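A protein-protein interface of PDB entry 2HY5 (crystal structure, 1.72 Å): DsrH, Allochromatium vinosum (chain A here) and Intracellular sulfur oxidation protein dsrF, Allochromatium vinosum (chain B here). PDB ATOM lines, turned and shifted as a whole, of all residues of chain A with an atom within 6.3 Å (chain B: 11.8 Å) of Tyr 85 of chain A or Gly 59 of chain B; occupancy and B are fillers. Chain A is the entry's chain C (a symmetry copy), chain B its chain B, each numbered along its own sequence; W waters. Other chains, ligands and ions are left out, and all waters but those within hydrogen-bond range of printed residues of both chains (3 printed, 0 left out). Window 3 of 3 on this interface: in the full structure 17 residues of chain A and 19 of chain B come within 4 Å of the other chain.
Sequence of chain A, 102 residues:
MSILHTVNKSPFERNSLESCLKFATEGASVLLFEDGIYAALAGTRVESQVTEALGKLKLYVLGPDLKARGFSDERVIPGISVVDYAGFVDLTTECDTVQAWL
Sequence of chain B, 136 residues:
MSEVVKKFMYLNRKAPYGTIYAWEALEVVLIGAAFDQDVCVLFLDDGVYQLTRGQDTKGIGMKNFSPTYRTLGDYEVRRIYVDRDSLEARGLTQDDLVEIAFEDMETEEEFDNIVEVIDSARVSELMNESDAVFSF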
ATOM      1  N   PHE A  33      -8.522  33.434  10.412  1.00  0.00           N
ATOM      2  CA  PHE A  33      -8.386  32.037  10.036  1.00  0.00           C
ATOM      3  C   PHE A  33      -6.967  31.792   9.537  1.00  0.00           C
ATOM      4  O   PHE A  33      -6.204  32.740   9.356  1.00  0.00           O
ATOM      5  CB  PHE A  33      -9.475  31.605   9.030  1.00  0.00           C
ATOM      6  CG  PHE A  33      -9.326  32.176   7.644  1.00  0.00           C
ATOM      7  CD1 PHE A  33      -9.369  33.548   7.419  1.00  0.00           C
ATOM      8  CD2 PHE A  33      -9.209  31.324   6.548  1.00  0.00           C
ATOM      9  CE1 PHE A  33      -9.301  34.062   6.125  1.00  0.00           C
ATOM     10  CE2 PHE A  33      -9.142  31.829   5.253  1.00  0.00           C
ATOM     11  CZ  PHE A  33      -9.188  33.200   5.040  1.00  0.00           C
ATOM     12  N   LEU A  62     -11.475  30.979  13.533  1.00  0.00           N
ATOM     13  CA  LEU A  62     -11.822  29.666  12.996  1.00  0.00           C
ATOM     14  C   LEU A  62     -11.256  28.538  13.858  1.00  0.00           C
ATOM     15  O   LEU A  62     -10.045  28.326  13.915  1.00  0.00           O
ATOM     16  CB  LEU A  62     -11.326  29.544  11.548  1.00  0.00           C
ATOM     17  CG  LEU A  62     -11.823  28.329  10.762  1.00  0.00           C
ATOM     18  CD1 LEU A  62     -13.342  28.368  10.608  1.00  0.00           C
ATOM     19  CD2 LEU A  62     -11.158  28.328   9.399  1.00  0.00           C
ATOM     20  N   PRO A  64     -11.139  25.226  13.569  1.00  0.00           N
ATOM     21  CA  PRO A  64     -10.293  24.215  12.930  1.00  0.00           C
ATOM     22  C   PRO A  64      -8.828  24.650  12.834  1.00  0.00           C
ATOM     23  O   PRO A  64      -7.925  23.847  13.076  1.00  0.00           O
ATOM     24  CB  PRO A  64     -10.950  24.039  11.566  1.00  0.00           C
ATOM     25  CG  PRO A  64     -12.400  24.220  11.886  1.00  0.00           C
ATOM     26  CD  PRO A  64     -12.370  25.442  12.786  1.00  0.00           C
ATOM     27  N   ASP A  65      -8.590  25.911  12.478  1.00  0.00           N
ATOM     28  CA  ASP A  65      -7.219  26.407  12.385  1.00  0.00           C
ATOM     29  C   ASP A  65      -6.616  26.573  13.779  1.00  0.00           C
ATOM     30  O   ASP A  65      -5.426  26.332  13.983  1.00  0.00           O
ATOM     31  CB  ASP A  65      -7.164  27.725  11.598  1.00  0.00           C
ATOM     32  CG  ASP A  65      -7.146  27.499  10.087  1.00  0.00           C
ATOM     33  OD1 ASP A  65      -6.364  26.633   9.633  1.00  0.00           O
ATOM     34  OD2 ASP A  65      -7.888  28.188   9.350  1.00  0.00           O
ATOM     35  N   LYS A  67      -7.296  24.765  16.493  1.00  0.00           N
ATOM     36  CA  LYS A  67      -6.958  23.427  16.965  1.00  0.00           C
ATOM     37  C   LYS A  67      -5.755  22.836  16.241  1.00  0.00           C
ATOM     38  O   LYS A  67      -4.919  22.171  16.848  1.00  0.00           O
ATOM     39  CB  LYS A  67      -8.147  22.474  16.783  1.00  0.00           C
ATOM     40  CG  LYS A  67      -9.482  22.956  17.315  1.00  0.00           C
ATOM     41  CD  LYS A  67     -10.573  21.972  16.904  1.00  0.00           C
ATOM     42  CE  LYS A  67     -11.965  22.599  16.896  1.00  0.00           C
ATOM     43  NZ  LYS A  67     -12.394  23.102  18.230  1.00  0.00           N
ATOM     44  N   VAL A  83     -15.743  29.784  15.662  1.00  0.00           N
ATOM     45  CA  VAL A  83     -16.666  29.228  14.676  1.00  0.00           C
ATOM     46  C   VAL A  83     -15.983  28.146  13.835  1.00  0.00           C
ATOM     47  O   VAL A  83     -14.757  28.061  13.799  1.00  0.00           O
ATOM     48  CB  VAL A  83     -17.172  30.321  13.715  1.00  0.00           C
ATOM     49  CG1 VAL A  83     -17.878  31.420  14.498  1.00  0.00           C
ATOM     50  CG2 VAL A  83     -16.000  30.898  12.923  1.00  0.00           C
ATOM     51  N   ASP A  84     -16.776  27.302  13.178  1.00  0.00           N
ATOM     52  CA  ASP A  84     -16.200  26.277  12.312  1.00  0.00           C
ATOM     53  C   ASP A  84     -16.416  26.750  10.883  1.00  0.00           C
ATOM     54  O   ASP A  84     -16.849  27.879  10.668  1.00  0.00           O
ATOM     55  CB  ASP A  84     -16.858  24.909  12.532  1.00  0.00           C
ATOM     56  CG  ASP A  84     -18.365  24.973  12.504  1.00  0.00           C
ATOM     57  OD1 ASP A  84     -18.915  25.916  11.899  1.00  0.00           O
ATOM     58  OD2 ASP A  84     -19.000  24.067  13.080  1.00  0.00           O
ATOM     59  N   TYR A  85     -16.117  25.912   9.900  1.00  0.00           N
ATOM     60  CA  TYR A  85     -16.298  26.349   8.520  1.00  0.00           C
ATOM     61  C   TYR A  85     -17.746  26.697   8.194  1.00  0.00           C
ATOM     62  O   TYR A  85     -18.005  27.621   7.420  1.00  0.00           O
ATOM     63  CB  TYR A  85     -15.758  25.297   7.549  1.00  0.00           C
ATOM     64  CG  TYR A  85     -14.246  25.335   7.423  1.00  0.00           C
ATOM     65  CD1 TYR A  85     -13.447  24.341   7.994  1.00  0.00           C
ATOM     66  CD2 TYR A  85     -13.614  26.376   6.746  1.00  0.00           C
ATOM     67  CE1 TYR A  85     -12.053  24.385   7.890  1.00  0.00           C
ATOM     68  CE2 TYR A  85     -12.224  26.431   6.635  1.00  0.00           C
ATOM     69  CZ  TYR A  85     -11.452  25.435   7.208  1.00  0.00           C
ATOM     70  OH  TYR A  85     -10.080  25.482   7.099  1.00  0.00           O
ATOM     71  N   ALA A  86     -18.693  25.971   8.783  1.00  0.00           N
ATOM     72  CA  ALA A  86     -20.098  26.267   8.540  1.00  0.00           C
ATOM     73  C   ALA A  86     -20.396  27.664   9.091  1.00  0.00           C
ATOM     74  O   ALA A  86     -21.150  28.423   8.492  1.00  0.00           O
ATOM     75  CB  ALA A  86     -20.988  25.220   9.216  1.00  0.00           C
ATOM     76  N   GLY A  87     -19.786  27.997  10.230  1.00  0.00           N
ATOM     77  CA  GLY A  87     -19.983  29.310  10.822  1.00  0.00           C
ATOM     78  C   GLY A  87     -19.368  30.400   9.961  1.00  0.00           C
ATOM     79  O   GLY A  87     -19.885  31.514   9.880  1.00  0.00           O
ATOM     80  N   PHE A  88     -18.247  30.067   9.326  1.00  0.00           N
ATOM     81  CA  PHE A  88     -17.522  30.973   8.437  1.00  0.00           C
ATOM     82  C   PHE A  88     -18.474  31.315   7.290  1.00  0.00           C
ATOM     83  O   PHE A  88     -18.650  32.478   6.927  1.00  0.00           O
ATOM     84  CB  PHE A  88     -16.264  30.238   7.940  1.00  0.00           C
ATOM     85  CG  PHE A  88     -15.322  31.065   7.091  1.00  0.00           C
ATOM     86  CD1 PHE A  88     -14.066  30.557   6.775  1.00  0.00           C
ATOM     87  CD2 PHE A  88     -15.689  32.304   6.569  1.00  0.00           C
ATOM     88  CE1 PHE A  88     -13.190  31.264   5.952  1.00  0.00           C
ATOM     89  CE2 PHE A  88     -14.822  33.017   5.745  1.00  0.00           C
ATOM     90  CZ  PHE A  88     -13.568  32.495   5.435  1.00  0.00           C
ATOM     91  N   VAL A  89     -19.104  30.289   6.732  1.00  0.00           N
ATOM     92  CA  VAL A  89     -20.053  30.493   5.645  1.00  0.00           C
ATOM     93  C   VAL A  89     -21.215  31.386   6.094  1.00  0.00           C
ATOM     94  O   VAL A  89     -21.607  32.300   5.370  1.00  0.00           O
ATOM     95  CB  VAL A  89     -20.616  29.151   5.137  1.00  0.00           C
ATOM     96  CG1 VAL A  89     -21.774  29.399   4.168  1.00  0.00           C
ATOM     97  CG2 VAL A  89     -19.518  28.368   4.445  1.00  0.00           C
ATOM     98  N   ASP A  90     -21.773  31.127   7.274  1.00  0.00           N
ATOM     99  CA  ASP A  90     -22.883  31.947   7.757  1.00  0.00           C
ATOM    100  C   ASP A  90     -22.474  33.407   7.927  1.00  0.00           C
ATOM    101  O   ASP A  90     -23.280  34.308   7.704  1.00  0.00           O
ATOM    102  CB  ASP A  90     -23.429  31.412   9.085  1.00  0.00           C
ATOM    103  CG  ASP A  90     -24.219  30.131   8.917  1.00  0.00           C
ATOM    104  OD1 ASP A  90     -24.817  29.934   7.839  1.00  0.00           O
ATOM    105  OD2 ASP A  90     -24.256  29.327   9.870  1.00  0.00           O
ATOM    106  N   PRO B  16       3.396  26.923  11.276  1.00  0.00           N
ATOM    107  CA  PRO B  16       3.016  25.731  10.517  1.00  0.00           C
ATOM    108  C   PRO B  16       1.617  25.827   9.904  1.00  0.00           C
ATOM    109  O   PRO B  16       0.792  26.639  10.333  1.00  0.00           O
ATOM    110  CB  PRO B  16       3.121  24.625  11.561  1.00  0.00           C
ATOM    111  CG  PRO B  16       2.657  25.316  12.795  1.00  0.00           C
ATOM    112  CD  PRO B  16       3.381  26.647  12.725  1.00  0.00           C
ATOM    113  N   TYR B  17       1.389  25.007   8.880  1.00  0.00           N
ATOM    114  CA  TYR B  17       0.114  24.896   8.171  1.00  0.00           C
ATOM    115  C   TYR B  17      -0.326  26.019   7.239  1.00  0.00           C
ATOM    116  O   TYR B  17      -0.854  25.743   6.164  1.00  0.00           O
ATOM    117  CB  TYR B  17      -0.998  24.585   9.174  1.00  0.00           C
ATOM    118  CG  TYR B  17      -0.699  23.355   9.987  1.00  0.00           C
ATOM    119  CD1 TYR B  17      -0.425  23.448  11.352  1.00  0.00           C
ATOM    120  CD2 TYR B  17      -0.633  22.096   9.384  1.00  0.00           C
ATOM    121  CE1 TYR B  17      -0.087  22.321  12.094  1.00  0.00           C
ATOM    122  CE2 TYR B  17      -0.295  20.964  10.121  1.00  0.00           C
ATOM    123  CZ  TYR B  17      -0.021  21.085  11.472  1.00  0.00           C
ATOM    124  OH  TYR B  17       0.346  19.974  12.195  1.00  0.00           O
ATOM    125  N   GLY B  18      -0.123  27.269   7.637  1.00  0.00           N
ATOM    126  CA  GLY B  18      -0.509  28.385   6.780  1.00  0.00           C
ATOM    127  C   GLY B  18       0.270  28.327   5.477  1.00  0.00           C
ATOM    128  O   GLY B  18      -0.213  28.744   4.415  1.00  0.00           O
ATOM    129  N   GLY B  54       0.062  19.358  21.304  1.00  0.00           N
ATOM    130  CA  GLY B  54      -1.367  19.148  21.130  1.00  0.00           C
ATOM    131  C   GLY B  54      -2.028  19.587  19.837  1.00  0.00           C
ATOM    132  O   GLY B  54      -3.222  19.890  19.822  1.00  0.00           O
ATOM    133  N   GLN B  55      -1.271  19.629  18.749  1.00  0.00           N
ATOM    134  CA  GLN B  55      -1.839  20.018  17.468  1.00  0.00           C
ATOM    135  C   GLN B  55      -2.802  18.926  17.001  1.00  0.00           C
ATOM    136  O   GLN B  55      -2.490  17.740  17.090  1.00  0.00           O
ATOM    137  CB  GLN B  55      -0.724  20.222  16.441  1.00  0.00           C
ATOM    138  CG  GLN B  55       0.112  21.469  16.678  1.00  0.00           C
ATOM    139  CD  GLN B  55       1.294  21.570  15.732  1.00  0.00           C
ATOM    140  OE1 GLN B  55       1.367  20.851  14.734  1.00  0.00           O
ATOM    141  NE2 GLN B  55       2.224  22.467  16.038  1.00  0.00           N
ATOM    142  N   ASP B  56      -3.978  19.337  16.528  1.00  0.00           N
ATOM    143  CA  ASP B  56      -5.012  18.419  16.034  1.00  0.00           C
ATOM    144  C   ASP B  56      -5.525  18.989  14.712  1.00  0.00           C
ATOM    145  O   ASP B  56      -6.264  19.973  14.696  1.00  0.00           O
ATOM    146  CB  ASP B  56      -6.156  18.321  17.045  1.00  0.00           C
ATOM    147  CG  ASP B  56      -7.288  17.425  16.568  1.00  0.00           C
ATOM    148  OD1 ASP B  56      -8.223  17.182  17.360  1.00  0.00           O
ATOM    149  OD2 ASP B  56      -7.247  16.964  15.407  1.00  0.00           O
ATOM    150  N   THR B  57      -5.152  18.347  13.610  1.00  0.00           N
ATOM    151  CA  THR B  57      -5.513  18.824  12.275  1.00  0.00           C
ATOM    152  C   THR B  57      -6.719  18.202  11.574  1.00  0.00           C
ATOM    153  O   THR B  57      -6.947  18.476  10.400  1.00  0.00           O
ATOM    154  CB  THR B  57      -4.323  18.665  11.329  1.00  0.00           C
ATOM    155  OG1 THR B  57      -4.028  17.267  11.187  1.00  0.00           O
ATOM    156  CG2 THR B  57      -3.098  19.382  11.893  1.00  0.00           C
ATOM    157  N   LYS B  58      -7.492  17.375  12.264  1.00  0.00           N
ATOM    158  CA  LYS B  58      -8.646  16.757  11.617  1.00  0.00           C
ATOM    159  C   LYS B  58      -9.658  17.779  11.089  1.00  0.00           C
ATOM    160  O   LYS B  58     -10.349  17.527  10.100  1.00  0.00           O
ATOM    161  CB  LYS B  58      -9.328  15.784  12.582  1.00  0.00           C
ATOM    162  CG  LYS B  58      -8.465  14.584  12.939  1.00  0.00           C
ATOM    163  CD  LYS B  58      -9.221  13.585  13.798  1.00  0.00           C
ATOM    164  CE  LYS B  58      -8.372  12.361  14.099  1.00  0.00           C
ATOM    165  NZ  LYS B  58      -9.110  11.358  14.916  1.00  0.00           N
ATOM    166  N   GLY B  59      -9.729  18.935  11.738  1.00  0.00           N
ATOM    167  CA  GLY B  59     -10.668  19.958  11.315  1.00  0.00           C
ATOM    168  C   GLY B  59     -10.297  20.705  10.045  1.00  0.00           C
ATOM    169  O   GLY B  59     -11.171  21.285   9.402  1.00  0.00           O
ATOM    170  N   ILE B  60      -9.017  20.706   9.676  1.00  0.00           N
ATOM    171  CA  ILE B  60      -8.591  21.412   8.472  1.00  0.00           C
ATOM    172  C   ILE B  60      -8.275  20.497   7.296  1.00  0.00           C
ATOM    173  O   ILE B  60      -7.825  20.963   6.252  1.00  0.00           O
ATOM    174  CB  ILE B  60      -7.362  22.325   8.739  1.00  0.00           C
ATOM    175  CG1 ILE B  60      -6.187  21.503   9.261  1.00  0.00           C
ATOM    176  CG2 ILE B  60      -7.731  23.420   9.723  1.00  0.00           C
ATOM    177  CD1 ILE B  60      -4.890  22.284   9.329  1.00  0.00           C
ATOM    178  N   GLY B  61      -8.509  19.200   7.474  1.00  0.00           N
ATOM    179  CA  GLY B  61      -8.275  18.243   6.408  1.00  0.00           C
ATOM    180  C   GLY B  61      -6.835  18.019   5.982  1.00  0.00           C
ATOM    181  O   GLY B  61      -6.582  17.642   4.839  1.00  0.00           O
ATOM    182  N   MET B  62      -5.893  18.246   6.892  1.00  0.00           N
ATOM    183  CA  MET B  62      -4.472  18.055   6.599  1.00  0.00           C
ATOM    184  C   MET B  62      -3.849  17.056   7.557  1.00  0.00           C
ATOM    185  O   MET B  62      -4.315  16.892   8.679  1.00  0.00           O
ATOM    186  CB  MET B  62      -3.696  19.360   6.754  1.00  0.00           C
ATOM    187  CG  MET B  62      -3.929  20.401   5.702  1.00  0.00           C
ATOM    188  SD  MET B  62      -2.788  21.751   6.028  1.00  0.00           S
ATOM    189  CE  MET B  62      -1.303  21.139   5.251  1.00  0.00           C
ATOM    190  N   LYS B  63      -2.779  16.404   7.118  1.00  0.00           N
ATOM    191  CA  LYS B  63      -2.090  15.451   7.974  1.00  0.00           C
ATOM    192  C   LYS B  63      -1.323  16.236   9.029  1.00  0.00           C
ATOM    193  O   LYS B  63      -0.740  17.283   8.742  1.00  0.00           O
ATOM    194  CB  LYS B  63      -1.109  14.601   7.168  1.00  0.00           C
ATOM    195  CG  LYS B  63      -0.304  13.637   8.026  1.00  0.00           C
ATOM    196  CD  LYS B  63       0.811  12.987   7.229  1.00  0.00           C
ATOM    197  CE  LYS B  63       1.695  12.126   8.116  1.00  0.00           C
ATOM    198  NZ  LYS B  63       2.904  11.646   7.387  1.00  0.00           N
ATOM    199  N   ASN B  64      -1.347  15.727  10.253  1.00  0.00           N
ATOM    200  CA  ASN B  64      -0.655  16.347  11.372  1.00  0.00           C
ATOM    201  C   ASN B  64       0.796  15.868  11.308  1.00  0.00           C
ATOM    202  O   ASN B  64       1.072  14.698  11.560  1.00  0.00           O
ATOM    203  CB  ASN B  64      -1.335  15.893  12.670  1.00  0.00           C
ATOM    204  CG  ASN B  64      -0.748  16.532  13.910  1.00  0.00           C
ATOM    205  OD1 ASN B  64      -1.342  16.460  14.986  1.00  0.00           O
ATOM    206  ND2 ASN B  64       0.419  17.148  13.778  1.00  0.00           N
ATOM    207  N   PHE B  65       1.723  16.757  10.953  1.00  0.00           N
ATOM    208  CA  PHE B  65       3.127  16.357  10.859  1.00  0.00           C
ATOM    209  C   PHE B  65       3.948  16.649  12.109  1.00  0.00           C
ATOM    210  O   PHE B  65       5.144  16.357  12.152  1.00  0.00           O
ATOM    211  CB  PHE B  65       3.807  17.002   9.640  1.00  0.00           C
ATOM    212  CG  PHE B  65       3.922  18.504   9.711  1.00  0.00           C
ATOM    213  CD1 PHE B  65       2.890  19.322   9.261  1.00  0.00           C
ATOM    214  CD2 PHE B  65       5.078  19.102  10.211  1.00  0.00           C
ATOM    215  CE1 PHE B  65       3.012  20.719   9.302  1.00  0.00           C
ATOM    216  CE2 PHE B  65       5.208  20.491  10.257  1.00  0.00           C
ATOM    217  CZ  PHE B  65       4.175  21.301   9.803  1.00  0.00           C
HETATM  218  O   HOH W   1      -8.118  21.162  13.010  1.00  0.00           O
HETATM  219  O   HOH W   2      -5.236  21.371  19.473  1.00  0.00           O
HETATM  220  O   HOH W   3      -8.031  24.042   5.596  1.00  0.00           O
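Among the printed residues, merely in contact across the chains: Pro 64 of chain A with Gly 59 of chain B, Pro 64 of chain A with Ile 60 of chain B, Asp 65 of chain A with Ile 60 of chain B, Lys 67 of chain A with Gln 55 of chain B and Tyr 85 of chain A with Gly 59 of chain B.
OH of Tyr 17 of chain B lies within hydrogen-bond range of OE1 of Gln 55 of chain B (2.9 Å).
The backbone carbonyl oxygen (O) of Gln 55 of chain B lies close to the side-chain amide oxygen (OD1) of Asn 64 of chain B, at 2.7 Å.
The backbone NH (N) of Lys 58 of chain B lies within hydrogen-bond range of the side-chain carboxylate (OD2) of Asp 56 of chain B, 3.2 Å away.
Water W2 lies within hydrogen-bond range of the backbone carbonyl oxygen of Gly 54 of chain B (2.5 Å) and the backbone carbonyl oxygen of Lys 67 of chain A (2.8 Å).
Water W1 lies within hydrogen-bond range of the backbone carbonyl oxygen of Pro 64 of chain A (2.7 Å), the backbone carbonyl oxygen of Asp 56 of chain B (2.8 Å), the backbone NH of Gly 59 of chain B (3.0 Å) and the backbone NH of Ile 60 of chain B (3.5 Å).
Water W3 bridges the side-chain hydroxyl of Tyr 85 of chain A (2.9 Å) and the backbone carbonyl oxygen of Ile 60 of chain B (3.2 Å).
Printed residues of chain A that touch a printed residue of chain B: Pro 64, Asp 65, Lys 67 and Tyr 85.
Hydrophobic or aromatic side chains of chain A that line the printed part of chain B: Pro 64 and Tyr 85.
Among the printed residues, 6 pairs touch across the chains.
Among the printed residues, no Asp or Glu carboxylate lies within 4 Å of a Lys or Arg side-chain nitrogen of the other chain.
The backbone NH of Asp 56 of chain B lies within hydrogen-bond range of the backbone carbonyl oxygen of Lys 67 of chain A (3.0 Å).
Of chain B, only Gly 59 (3.5 Å) and Ile 60 (3.4 Å) come within 4 Å of Pro 64 of chain A.
Printed residues of chain B within 4 Å of Asp 65 of chain A: Ile 60.
Of the printed residues of chain B, Lys 67 of chain A touches Gln 55 (3.8 Å) and Asp 56 (3.0 Å).
No residue of chain B comes within 4 Å of Val 83 of chain A.
Tyr 85 of chain A touches just one residue of chain B: Gly 59.
Phe 88 of chain A touches none of the printed residues of chain B.
Printed residues of chain A within 4 Å of Asp 56 of chain B: Lys 67 (3.0 Å).
Gly 59 of chain B touches just these residues of chain A: Pro 64 and Tyr 85.
The nearest residue of chain B that does not touch Tyr 85 of chain A is Ile 60 of chain B (4.1 Å).
The nearest residue of chain A that does not touch Gly 59 of chain B is Lys 67 of chain A (5.9 Å).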
